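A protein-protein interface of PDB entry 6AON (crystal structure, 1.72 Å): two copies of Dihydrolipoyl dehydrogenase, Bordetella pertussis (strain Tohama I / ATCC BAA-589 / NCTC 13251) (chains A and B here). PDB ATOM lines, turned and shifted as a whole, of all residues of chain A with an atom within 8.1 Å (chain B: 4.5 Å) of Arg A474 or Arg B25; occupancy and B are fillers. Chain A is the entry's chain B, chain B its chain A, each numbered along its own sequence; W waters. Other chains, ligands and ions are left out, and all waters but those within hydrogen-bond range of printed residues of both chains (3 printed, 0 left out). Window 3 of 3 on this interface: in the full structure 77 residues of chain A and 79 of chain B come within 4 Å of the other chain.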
ATOM      1  N   ASP A 418     -14.603  -8.715 -18.181  1.00  0.00           N
ATOM      2  CA  ASP A 418     -16.030  -8.782 -17.831  1.00  0.00           C
ATOM      3  C   ASP A 418     -16.331  -9.802 -16.726  1.00  0.00           C
ATOM      4  O   ASP A 418     -17.480 -10.015 -16.409  1.00  0.00           O
ATOM      5  CB  ASP A 418     -16.914  -9.081 -19.057  1.00  0.00           C
ATOM      6  CG  ASP A 418     -18.356  -8.605 -18.877  1.00  0.00           C
ATOM      7  OD1 ASP A 418     -18.569  -7.514 -18.290  1.00  0.00           O
ATOM      8  OD2 ASP A 418     -19.280  -9.303 -19.357  1.00  0.00           O
ATOM      9  N   ALA A 447     -20.407 -10.600 -16.343  1.00  0.00           N
ATOM     10  CA  ALA A 447     -21.617  -9.784 -16.233  1.00  0.00           C
ATOM     11  C   ALA A 447     -22.542 -10.121 -17.391  1.00  0.00           C
ATOM     12  O   ALA A 447     -23.731 -10.291 -17.202  1.00  0.00           O
ATOM     13  CB  ALA A 447     -21.271  -8.299 -16.274  1.00  0.00           C
ATOM     14  N   GLU A 448     -21.984 -10.226 -18.595  1.00  0.00           N
ATOM     15  CA  GLU A 448     -22.798 -10.550 -19.762  1.00  0.00           C
ATOM     16  C   GLU A 448     -23.525 -11.904 -19.621  1.00  0.00           C
ATOM     17  O   GLU A 448     -24.627 -12.062 -20.147  1.00  0.00           O
ATOM     18  CB  GLU A 448     -21.968 -10.493 -21.046  1.00  0.00           C
ATOM     19  CG  GLU A 448     -22.810 -10.629 -22.302  1.00  0.00           C
ATOM     20  CD  GLU A 448     -22.006 -10.471 -23.573  1.00  0.00           C
ATOM     21  OE1 GLU A 448     -20.793 -10.187 -23.480  1.00  0.00           O
ATOM     22  OE2 GLU A 448     -22.592 -10.631 -24.662  1.00  0.00           O
ATOM     23  N   ASP A 449     -22.915 -12.865 -18.906  1.00  0.00           N
ATOM     24  CA  ASP A 449     -23.564 -14.171 -18.656  1.00  0.00           C
ATOM     25  C   ASP A 449     -24.853 -13.991 -17.845  1.00  0.00           C
ATOM     26  O   ASP A 449     -25.878 -14.581 -18.176  1.00  0.00           O
ATOM     27  CB  ASP A 449     -22.637 -15.150 -17.928  1.00  0.00           C
ATOM     28  CG  ASP A 449     -21.411 -15.522 -18.738  1.00  0.00           C
ATOM     29  OD1 ASP A 449     -21.479 -15.494 -19.995  1.00  0.00           O
ATOM     30  OD2 ASP A 449     -20.377 -15.854 -18.116  1.00  0.00           O
ATOM     31  N   ILE A 450     -24.807 -13.153 -16.812  1.00  0.00           N
ATOM     32  CA  ILE A 450     -25.992 -12.886 -15.994  1.00  0.00           C
ATOM     33  C   ILE A 450     -27.027 -12.197 -16.849  1.00  0.00           C
ATOM     34  O   ILE A 450     -28.196 -12.560 -16.820  1.00  0.00           O
ATOM     35  CB  ILE A 450     -25.685 -11.973 -14.787  1.00  0.00           C
ATOM     36  CG1 ILE A 450     -24.685 -12.646 -13.847  1.00  0.00           C
ATOM     37  CG2 ILE A 450     -26.964 -11.643 -14.009  1.00  0.00           C
ATOM     38  CD1 ILE A 450     -24.286 -11.775 -12.681  1.00  0.00           C
ATOM     39  N   ALA A 451     -26.580 -11.194 -17.596  1.00  0.00           N
ATOM     40  CA  ALA A 451     -27.447 -10.406 -18.476  1.00  0.00           C
ATOM     41  C   ALA A 451     -28.172 -11.253 -19.508  1.00  0.00           C
ATOM     42  O   ALA A 451     -29.287 -10.918 -19.905  1.00  0.00           O
ATOM     43  CB  ALA A 451     -26.623  -9.339 -19.185  1.00  0.00           C
ATOM     44  N   ARG A 452     -27.543 -12.342 -19.943  1.00  0.00           N
ATOM     45  CA  ARG A 452     -28.138 -13.209 -20.961  1.00  0.00           C
ATOM     46  C   ARG A 452     -28.851 -14.462 -20.433  1.00  0.00           C
ATOM     47  O   ARG A 452     -29.343 -15.285 -21.217  1.00  0.00           O
ATOM     48  CB  ARG A 452     -27.093 -13.537 -22.037  1.00  0.00           C
ATOM     49  CG  ARG A 452     -26.681 -12.295 -22.843  1.00  0.00           C
ATOM     50  CD  ARG A 452     -25.623 -12.603 -23.899  1.00  0.00           C
ATOM     51  NE  ARG A 452     -25.315 -11.428 -24.730  1.00  0.00           N
ATOM     52  CZ  ARG A 452     -26.063 -11.012 -25.752  1.00  0.00           C
ATOM     53  NH1 ARG A 452     -25.699  -9.934 -26.434  1.00  0.00           N
ATOM     54  NH2 ARG A 452     -27.194 -11.647 -26.079  1.00  0.00           N
ATOM     55  N   LYS A 465     -30.165  -9.335 -12.970  1.00  0.00           N
ATOM     56  CA  LYS A 465     -30.000  -9.362 -14.427  1.00  0.00           C
ATOM     57  C   LYS A 465     -29.857  -7.937 -14.968  1.00  0.00           C
ATOM     58  O   LYS A 465     -28.963  -7.648 -15.754  1.00  0.00           O
ATOM     59  CB  LYS A 465     -31.211 -10.041 -15.081  1.00  0.00           C
ATOM     60  CG  LYS A 465     -31.224 -10.030 -16.607  1.00  0.00           C
ATOM     61  CD  LYS A 465     -32.590 -10.438 -17.140  1.00  0.00           C
ATOM     62  CE  LYS A 465     -32.695 -10.336 -18.651  1.00  0.00           C
ATOM     63  NZ  LYS A 465     -31.992 -11.418 -19.389  1.00  0.00           N
ATOM     64  N   GLU A 466     -30.761  -7.045 -14.562  1.00  0.00           N
ATOM     65  CA  GLU A 466     -30.720  -5.667 -15.037  1.00  0.00           C
ATOM     66  C   GLU A 466     -29.446  -4.951 -14.585  1.00  0.00           C
ATOM     67  O   GLU A 466     -28.869  -4.173 -15.355  1.00  0.00           O
ATOM     68  CB  GLU A 466     -31.965  -4.887 -14.601  1.00  0.00           C
ATOM     69  CG  GLU A 466     -33.305  -5.342 -15.204  1.00  0.00           C
ATOM     70  CD  GLU A 466     -33.582  -4.884 -16.637  1.00  0.00           C
ATOM     71  OE1 GLU A 466     -32.903  -3.978 -17.163  1.00  0.00           O
ATOM     72  OE2 GLU A 466     -34.523  -5.441 -17.255  1.00  0.00           O
ATOM     73  N   ALA A 467     -29.008  -5.202 -13.347  1.00  0.00           N
ATOM     74  CA  ALA A 467     -27.748  -4.608 -12.844  1.00  0.00           C
ATOM     75  C   ALA A 467     -26.605  -5.045 -13.754  1.00  0.00           C
ATOM     76  O   ALA A 467     -25.734  -4.255 -14.088  1.00  0.00           O
ATOM     77  CB  ALA A 467     -27.474  -5.047 -11.424  1.00  0.00           C
ATOM     78  N   ALA A 468     -26.617  -6.318 -14.150  1.00  0.00           N
ATOM     79  CA  ALA A 468     -25.592  -6.844 -15.058  1.00  0.00           C
ATOM     80  C   ALA A 468     -25.690  -6.175 -16.443  1.00  0.00           C
ATOM     81  O   ALA A 468     -24.669  -5.843 -17.059  1.00  0.00           O
ATOM     82  CB  ALA A 468     -25.715  -8.352 -15.171  1.00  0.00           C
ATOM     83  N   LEU A 469     -26.910  -5.958 -16.925  1.00  0.00           N
ATOM     84  CA  LEU A 469     -27.096  -5.256 -18.192  1.00  0.00           C
ATOM     85  C   LEU A 469     -26.551  -3.843 -18.076  1.00  0.00           C
ATOM     86  O   LEU A 469     -25.963  -3.322 -19.041  1.00  0.00           O
ATOM     87  CB  LEU A 469     -28.572  -5.242 -18.621  1.00  0.00           C
ATOM     88  CG  LEU A 469     -29.142  -6.545 -19.172  1.00  0.00           C
ATOM     89  CD1 LEU A 469     -30.661  -6.491 -19.175  1.00  0.00           C
ATOM     90  CD2 LEU A 469     -28.607  -6.842 -20.564  1.00  0.00           C
ATOM     91  N   ALA A 470     -26.706  -3.234 -16.891  1.00  0.00           N
ATOM     92  CA  ALA A 470     -26.213  -1.867 -16.633  1.00  0.00           C
ATOM     93  C   ALA A 470     -24.695  -1.768 -16.723  1.00  0.00           C
ATOM     94  O   ALA A 470     -24.161  -0.703 -17.048  1.00  0.00           O
ATOM     95  CB  ALA A 470     -26.688  -1.341 -15.287  1.00  0.00           C
ATOM     96  N   VAL A 471     -23.997  -2.871 -16.427  1.00  0.00           N
ATOM     97  CA  VAL A 471     -22.529  -2.911 -16.577  1.00  0.00           C
ATOM     98  C   VAL A 471     -22.143  -2.530 -18.001  1.00  0.00           C
ATOM     99  O   VAL A 471     -21.145  -1.828 -18.197  1.00  0.00           O
ATOM    100  CB  VAL A 471     -21.929  -4.301 -16.217  1.00  0.00           C
ATOM    101  CG1 VAL A 471     -20.449  -4.416 -16.625  1.00  0.00           C
ATOM    102  CG2 VAL A 471     -22.089  -4.567 -14.732  1.00  0.00           C
ATOM    103  N   ASP A 472     -22.966  -2.950 -18.975  1.00  0.00           N
ATOM    104  CA  ASP A 472     -22.750  -2.679 -20.399  1.00  0.00           C
ATOM    105  C   ASP A 472     -23.638  -1.526 -20.916  1.00  0.00           C
ATOM    106  O   ASP A 472     -23.877  -1.413 -22.137  1.00  0.00           O
ATOM    107  CB  ASP A 472     -23.021  -3.965 -21.209  1.00  0.00           C
ATOM    108  CG  ASP A 472     -22.456  -3.916 -22.623  1.00  0.00           C
ATOM    109  OD1 ASP A 472     -21.368  -3.339 -22.812  1.00  0.00           O
ATOM    110  OD2 ASP A 472     -23.063  -4.522 -23.535  1.00  0.00           O
ATOM    111  N   LYS A 473     -24.140  -0.697 -19.991  1.00  0.00           N
ATOM    112  CA  LYS A 473     -24.970   0.476 -20.307  1.00  0.00           C
ATOM    113  C   LYS A 473     -26.182   0.133 -21.177  1.00  0.00           C
ATOM    114  O   LYS A 473     -26.532   0.894 -22.099  1.00  0.00           O
ATOM    115  CB  LYS A 473     -24.118   1.517 -21.042  1.00  0.00           C
ATOM    116  CG  LYS A 473     -22.845   1.961 -20.343  1.00  0.00           C
ATOM    117  CD  LYS A 473     -23.098   3.001 -19.272  1.00  0.00           C
ATOM    118  CE  LYS A 473     -21.791   3.681 -18.851  1.00  0.00           C
ATOM    119  NZ  LYS A 473     -22.038   4.826 -17.927  1.00  0.00           N
ATOM    120  N   ARG A 474     -26.820  -1.003 -20.891  1.00  0.00           N
ATOM    121  CA  ARG A 474     -27.972  -1.418 -21.685  1.00  0.00           C
ATOM    122  C   ARG A 474     -29.088  -2.038 -20.858  1.00  0.00           C
ATOM    123  O   ARG A 474     -29.662  -3.050 -21.239  1.00  0.00           O
ATOM    124  CB  ARG A 474     -27.541  -2.329 -22.856  1.00  0.00           C
ATOM    125  CG  ARG A 474     -26.917  -3.669 -22.470  1.00  0.00           C
ATOM    126  CD  ARG A 474     -26.360  -4.345 -23.710  1.00  0.00           C
ATOM    127  NE  ARG A 474     -25.899  -5.719 -23.474  1.00  0.00           N
ATOM    128  CZ  ARG A 474     -26.636  -6.820 -23.638  1.00  0.00           C
ATOM    129  NH1 ARG A 474     -27.916  -6.751 -24.016  1.00  0.00           N
ATOM    130  NH2 ARG A 474     -26.095  -8.013 -23.413  1.00  0.00           N
ATOM    131  N   THR A 475     -29.390  -1.416 -19.715  1.00  0.00           N
ATOM    132  CA  THR A 475     -30.521  -1.859 -18.917  1.00  0.00           C
ATOM    133  C   THR A 475     -31.751  -1.689 -19.809  1.00  0.00           C
ATOM    134  O   THR A 475     -31.841  -0.745 -20.604  1.00  0.00           O
ATOM    135  CB  THR A 475     -30.738  -1.030 -17.626  1.00  0.00           C
ATOM    136  OG1 THR A 475     -30.969   0.345 -17.960  1.00  0.00           O
ATOM    137  CG2 THR A 475     -29.570  -1.102 -16.762  1.00  0.00           C
ATOM    138  N   LEU A 476     -32.673  -2.627 -19.696  1.00  0.00           N
ATOM    139  CA  LEU A 476     -33.911  -2.606 -20.469  1.00  0.00           C
ATOM    140  C   LEU A 476     -35.051  -1.909 -19.736  1.00  0.00           C
ATOM    141  O   LEU A 476     -35.858  -1.221 -20.368  1.00  0.00           O
ATOM    142  CB  LEU A 476     -34.337  -4.048 -20.772  1.00  0.00           C
ATOM    143  CG  LEU A 476     -33.456  -4.840 -21.732  1.00  0.00           C
ATOM    144  CD1 LEU A 476     -33.722  -6.333 -21.571  1.00  0.00           C
ATOM    145  CD2 LEU A 476     -33.699  -4.374 -23.158  1.00  0.00           C
ATOM    146  N   ASN A 477     -35.100  -2.046 -18.404  1.00  0.00           N
ATOM    147  CA  ASN A 477     -36.219  -1.511 -17.619  1.00  0.00           C
ATOM    148  C   ASN A 477     -35.943  -0.322 -16.699  1.00  0.00           C
ATOM    149  O   ASN A 477     -36.742  -0.034 -15.808  1.00  0.00           O
ATOM    150  CB  ASN A 477     -36.891  -2.677 -16.884  1.00  0.00           C
ATOM    151  CG  ASN A 477     -37.677  -3.548 -17.835  1.00  0.00           C
ATOM    152  OD1 ASN A 477     -38.709  -3.122 -18.358  1.00  0.00           O
ATOM    153  ND2 ASN A 477     -37.184  -4.744 -18.097  1.00  0.00           N
ATOM    154  N   PHE A 478     -34.828   0.366 -16.951  1.00  0.00           N
ATOM    155  CA  PHE A 478     -34.477   1.599 -16.253  1.00  0.00           C
ATOM    156  C   PHE A 478     -33.718   2.467 -17.247  1.00  0.00           C
ATOM    157  O   PHE A 478     -33.101   1.948 -18.170  1.00  0.00           O
ATOM    158  CB  PHE A 478     -33.636   1.334 -15.000  1.00  0.00           C
ATOM    159  CG  PHE A 478     -33.388   2.567 -14.158  1.00  0.00           C
ATOM    160  CD1 PHE A 478     -34.437   3.172 -13.472  1.00  0.00           C
ATOM    161  CD2 PHE A 478     -32.103   3.095 -14.019  1.00  0.00           C
ATOM    162  CE1 PHE A 478     -34.217   4.292 -12.680  1.00  0.00           C
ATOM    163  CE2 PHE A 478     -31.879   4.219 -13.226  1.00  0.00           C
ATOM    164  CZ  PHE A 478     -32.941   4.817 -12.562  1.00  0.00           C
ATOM    165  OXT PHE A 478     -33.733   3.695 -17.185  1.00  0.00           O
ATOM    166  N   ILE B  21     -40.053  -4.790 -25.132  1.00  0.00           N
ATOM    167  CA  ILE B  21     -38.642  -5.196 -24.983  1.00  0.00           C
ATOM    168  C   ILE B  21     -37.948  -5.315 -26.349  1.00  0.00           C
ATOM    169  O   ILE B  21     -36.788  -4.880 -26.497  1.00  0.00           O
ATOM    170  CB  ILE B  21     -38.497  -6.484 -24.168  1.00  0.00           C
ATOM    171  CG1 ILE B  21     -38.886  -6.235 -22.697  1.00  0.00           C
ATOM    172  CG2 ILE B  21     -37.079  -7.031 -24.237  1.00  0.00           C
ATOM    173  CD1 ILE B  21     -37.989  -5.270 -21.939  1.00  0.00           C
ATOM    174  N   ALA B  22     -38.615  -5.902 -27.347  1.00  0.00           N
ATOM    175  CA  ALA B  22     -38.000  -5.990 -28.684  1.00  0.00           C
ATOM    176  C   ALA B  22     -37.701  -4.573 -29.214  1.00  0.00           C
ATOM    177  O   ALA B  22     -36.646  -4.309 -29.800  1.00  0.00           O
ATOM    178  CB  ALA B  22     -38.900  -6.750 -29.650  1.00  0.00           C
ATOM    179  N   ALA B  23     -38.636  -3.657 -28.996  1.00  0.00           N
ATOM    180  CA  ALA B  23     -38.467  -2.284 -29.481  1.00  0.00           C
ATOM    181  C   ALA B  23     -37.274  -1.600 -28.815  1.00  0.00           C
ATOM    182  O   ALA B  23     -36.433  -0.973 -29.479  1.00  0.00           O
ATOM    183  CB  ALA B  23     -39.731  -1.484 -29.221  1.00  0.00           C
ATOM    184  N   ILE B  24     -37.200  -1.739 -27.503  1.00  0.00           N
ATOM    185  CA  ILE B  24     -36.107  -1.132 -26.740  1.00  0.00           C
ATOM    186  C   ILE B  24     -34.767  -1.706 -27.181  1.00  0.00           C
ATOM    187  O   ILE B  24     -33.821  -0.955 -27.472  1.00  0.00           O
ATOM    188  CB  ILE B  24     -36.313  -1.307 -25.219  1.00  0.00           C
ATOM    189  CG1 ILE B  24     -37.459  -0.393 -24.750  1.00  0.00           C
ATOM    190  CG2 ILE B  24     -35.031  -0.944 -24.471  1.00  0.00           C
ATOM    191  CD1 ILE B  24     -37.942  -0.640 -23.331  1.00  0.00           C
ATOM    192  N   ARG B  25     -34.690  -3.027 -27.271  1.00  0.00           N
ATOM    193  CA  ARG B  25     -33.443  -3.684 -27.661  1.00  0.00           C
ATOM    194  C   ARG B  25     -32.996  -3.264 -29.070  1.00  0.00           C
ATOM    195  O   ARG B  25     -31.808  -3.017 -29.297  1.00  0.00           O
ATOM    196  CB  ARG B  25     -33.592  -5.201 -27.622  1.00  0.00           C
ATOM    197  CG  ARG B  25     -32.273  -5.943 -27.811  1.00  0.00           C
ATOM    198  CD  ARG B  25     -31.429  -5.877 -26.558  1.00  0.00           C
ATOM    199  NE  ARG B  25     -30.103  -6.440 -26.812  1.00  0.00           N
ATOM    200  CZ  ARG B  25     -28.982  -5.751 -27.015  1.00  0.00           C
ATOM    201  NH1 ARG B  25     -28.957  -4.427 -26.920  1.00  0.00           N
ATOM    202  NH2 ARG B  25     -27.841  -6.406 -27.267  1.00  0.00           N
ATOM    203  N   ALA B  26     -33.946  -3.195 -29.995  1.00  0.00           N
ATOM    204  CA  ALA B  26     -33.654  -2.765 -31.383  1.00  0.00           C
ATOM    205  C   ALA B  26     -33.080  -1.345 -31.394  1.00  0.00           C
ATOM    206  O   ALA B  26     -32.155  -1.045 -32.152  1.00  0.00           O
ATOM    207  CB  ALA B  26     -34.915  -2.826 -32.226  1.00  0.00           C
ATOM    208  N   ALA B  27     -33.648  -0.470 -30.560  1.00  0.00           N
ATOM    209  CA  ALA B  27     -33.172   0.910 -30.445  1.00  0.00           C
ATOM    210  C   ALA B  27     -31.750   0.963 -29.855  1.00  0.00           C
ATOM    211  O   ALA B  27     -30.890   1.709 -30.348  1.00  0.00           O
ATOM    212  CB  ALA B  27     -34.146   1.739 -29.618  1.00  0.00           C
ATOM    213  N   GLN B  28     -31.485   0.144 -28.838  1.00  0.00           N
ATOM    214  CA  GLN B  28     -30.149   0.056 -28.233  1.00  0.00           C
ATOM    215  C   GLN B  28     -29.106  -0.331 -29.264  1.00  0.00           C
ATOM    216  O   GLN B  28     -27.974   0.193 -29.257  1.00  0.00           O
ATOM    217  CB  GLN B  28     -30.130  -0.986 -27.109  1.00  0.00           C
ATOM    218  CG  GLN B  28     -30.889  -0.595 -25.854  1.00  0.00           C
ATOM    219  CD  GLN B  28     -30.873  -1.687 -24.800  1.00  0.00           C
ATOM    220  OE1 GLN B  28     -30.658  -2.869 -25.109  1.00  0.00           O
ATOM    221  NE2 GLN B  28     -31.104  -1.303 -23.552  1.00  0.00           N
ATOM    222  N   LEU B  29     -29.500  -1.246 -30.161  1.00  0.00           N
ATOM    223  CA  LEU B  29     -28.640  -1.721 -31.266  1.00  0.00           C
ATOM    224  C   LEU B  29     -28.459  -0.684 -32.400  1.00  0.00           C
ATOM    225  O   LEU B  29     -27.797  -0.962 -33.402  1.00  0.00           O
ATOM    226  CB  LEU B  29     -29.162  -3.065 -31.797  1.00  0.00           C
ATOM    227  CG  LEU B  29     -29.031  -4.201 -30.772  1.00  0.00           C
ATOM    228  CD1 LEU B  29     -29.983  -5.354 -31.063  1.00  0.00           C
ATOM    229  CD2 LEU B  29     -27.588  -4.686 -30.651  1.00  0.00           C
ATOM    230  N   VAL B 341     -35.881  -9.844 -27.473  1.00  0.00           N
ATOM    231  CA  VAL B 341     -34.458  -9.543 -27.477  1.00  0.00           C
ATOM    232  C   VAL B 341     -33.741 -10.320 -28.585  1.00  0.00           C
ATOM    233  O   VAL B 341     -32.929  -9.753 -29.320  1.00  0.00           O
ATOM    234  CB  VAL B 341     -33.802  -9.904 -26.129  1.00  0.00           C
ATOM    235  CG1 VAL B 341     -32.279  -9.839 -26.220  1.00  0.00           C
ATOM    236  CG2 VAL B 341     -34.323  -8.996 -25.017  1.00  0.00           C
ATOM    237  N   ALA B 344     -34.525  -8.849 -32.096  1.00  0.00           N
ATOM    238  CA  ALA B 344     -33.831  -7.563 -32.310  1.00  0.00           C
ATOM    239  C   ALA B 344     -32.356  -7.805 -32.571  1.00  0.00           C
ATOM    240  O   ALA B 344     -31.763  -7.178 -33.464  1.00  0.00           O
ATOM    241  CB  ALA B 344     -34.011  -6.614 -31.130  1.00  0.00           C
ATOM    242  N   GLU B 345     -31.775  -8.751 -31.833  1.00  0.00           N
ATOM    243  CA  GLU B 345     -30.373  -9.075 -32.017  1.00  0.00           C
ATOM    244  C   GLU B 345     -30.114  -9.709 -33.402  1.00  0.00           C
ATOM    245  O   GLU B 345     -29.120  -9.375 -34.067  1.00  0.00           O
ATOM    246  CB  GLU B 345     -29.844  -9.910 -30.840  1.00  0.00           C
ATOM    247  CG  GLU B 345     -29.726  -9.069 -29.555  1.00  0.00           C
ATOM    248  CD  GLU B 345     -29.241  -9.828 -28.329  1.00  0.00           C
ATOM    249  OE1 GLU B 345     -28.981 -11.051 -28.428  1.00  0.00           O
ATOM    250  OE2 GLU B 345     -29.094  -9.184 -27.248  1.00  0.00           O
HETATM  251  O   HOH W   1     -31.109   1.407 -23.041  1.00  0.00           O
HETATM  252  O   HOH W   2     -30.028  -4.846 -23.450  1.00  0.00           O
HETATM  253  O   HOH W   3     -28.911  -9.232 -24.568  1.00  0.00           O
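Printed residues of chain B within 4 Å of Arg A474: Arg B25 (3.3 Å) and Gln B28 (3.2 Å).
Of chain A, only Arg A474 (3.3 Å) comes within 4 Å of Arg B25.
No residue of chain A comes within 4 Å of Ala B26.
Printed residues of chain B within 4 Å of Asn A477: Ile B21.
Of the printed residues of chain B, Leu A476 touches Ile B24 and Gln B28.
Of the printed residues of chain B, Arg A452 touches Glu B345 (3.0 Å).
Ala B22 touches none of the printed residues of chain A.
Ala B23 touches none of the printed residues of chain A.
The nearest residue of chain A that does not touch Arg B25 is Arg A452 (4.2 Å).
The side-chain amide nitrogen (NE2) of Gln B28 sits at hydrogen-bond distance from the backbone carbonyl oxygen (O) of Arg A474, at 3.2 Å.
NE2 of Gln B28 lies within hydrogen-bond range of O of Thr A475, at 3.1 Å.
OE1 of Glu B345 lies within salt-bridge range of NH2 of Arg A452 (3.0 Å).
The guanidinium group of Arg A474 lies close to the guanidinium group of Arg B25 (3.3 Å).
Leu A476 touches Ile B24 (O to CD1, 3.7 Å).
Gln B28 touches Leu A476 (OE1 to CD2, 3.9 Å).
Ile B21 touches Asn A477 (CD1 to ND2, 3.96 Å).
Of the 12 printed residues of chain B, 5 touch a printed residue of chain A.
Hydrophobic or aromatic side chains of chain A within 4 Å of the printed part of chain B: Leu A476.
Along chain A the printed residues that touch a printed residue of chain B span positions 452 to 477.
Among the printed residues, 7 pairs touch across the chains.
No position is printed for both chains.
Of the 7 pairs that touch across the chains among the printed residues, none has its exchanged pair printed and touching as well.
Water W2 bridges OE1 of Gln B28 (2.7 Å) and O of Arg A474 (2.9 Å).
Water W3 lies within hydrogen-bond range of the side-chain carboxylate of Glu B345 (2.7 Å), the guanidinium group of Arg A474 (2.7 Å) and the guanidinium group of Arg A452 (3.3 Å).
Water W1 bridges NE2 of Gln B28 (2.8 Å) and O of Thr A475 (3.3 Å).
OE1 of Gln B28 is in hydrogen-bond range of NH1 of Arg B25, at 2.9 Å.
NE of Arg B25 is in salt-bridge range of OE2 of Glu B345 (3.0 Å).
The side-chain carboxylate of Glu A448 is in salt-bridge range of the guanidinium group of Arg A452 (2.8 Å).
OE1 of Glu A466 lies within hydrogen-bond range of N of Leu A476.
The side-chain carboxylate (OE2) of Glu A466 lies within hydrogen-bond range of the side-chain amide nitrogen (ND2) of Asn A477, 2.9 Å away.
OG1 of Thr A475 is in hydrogen-bond range of O of Phe A478 (2.7 Å).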
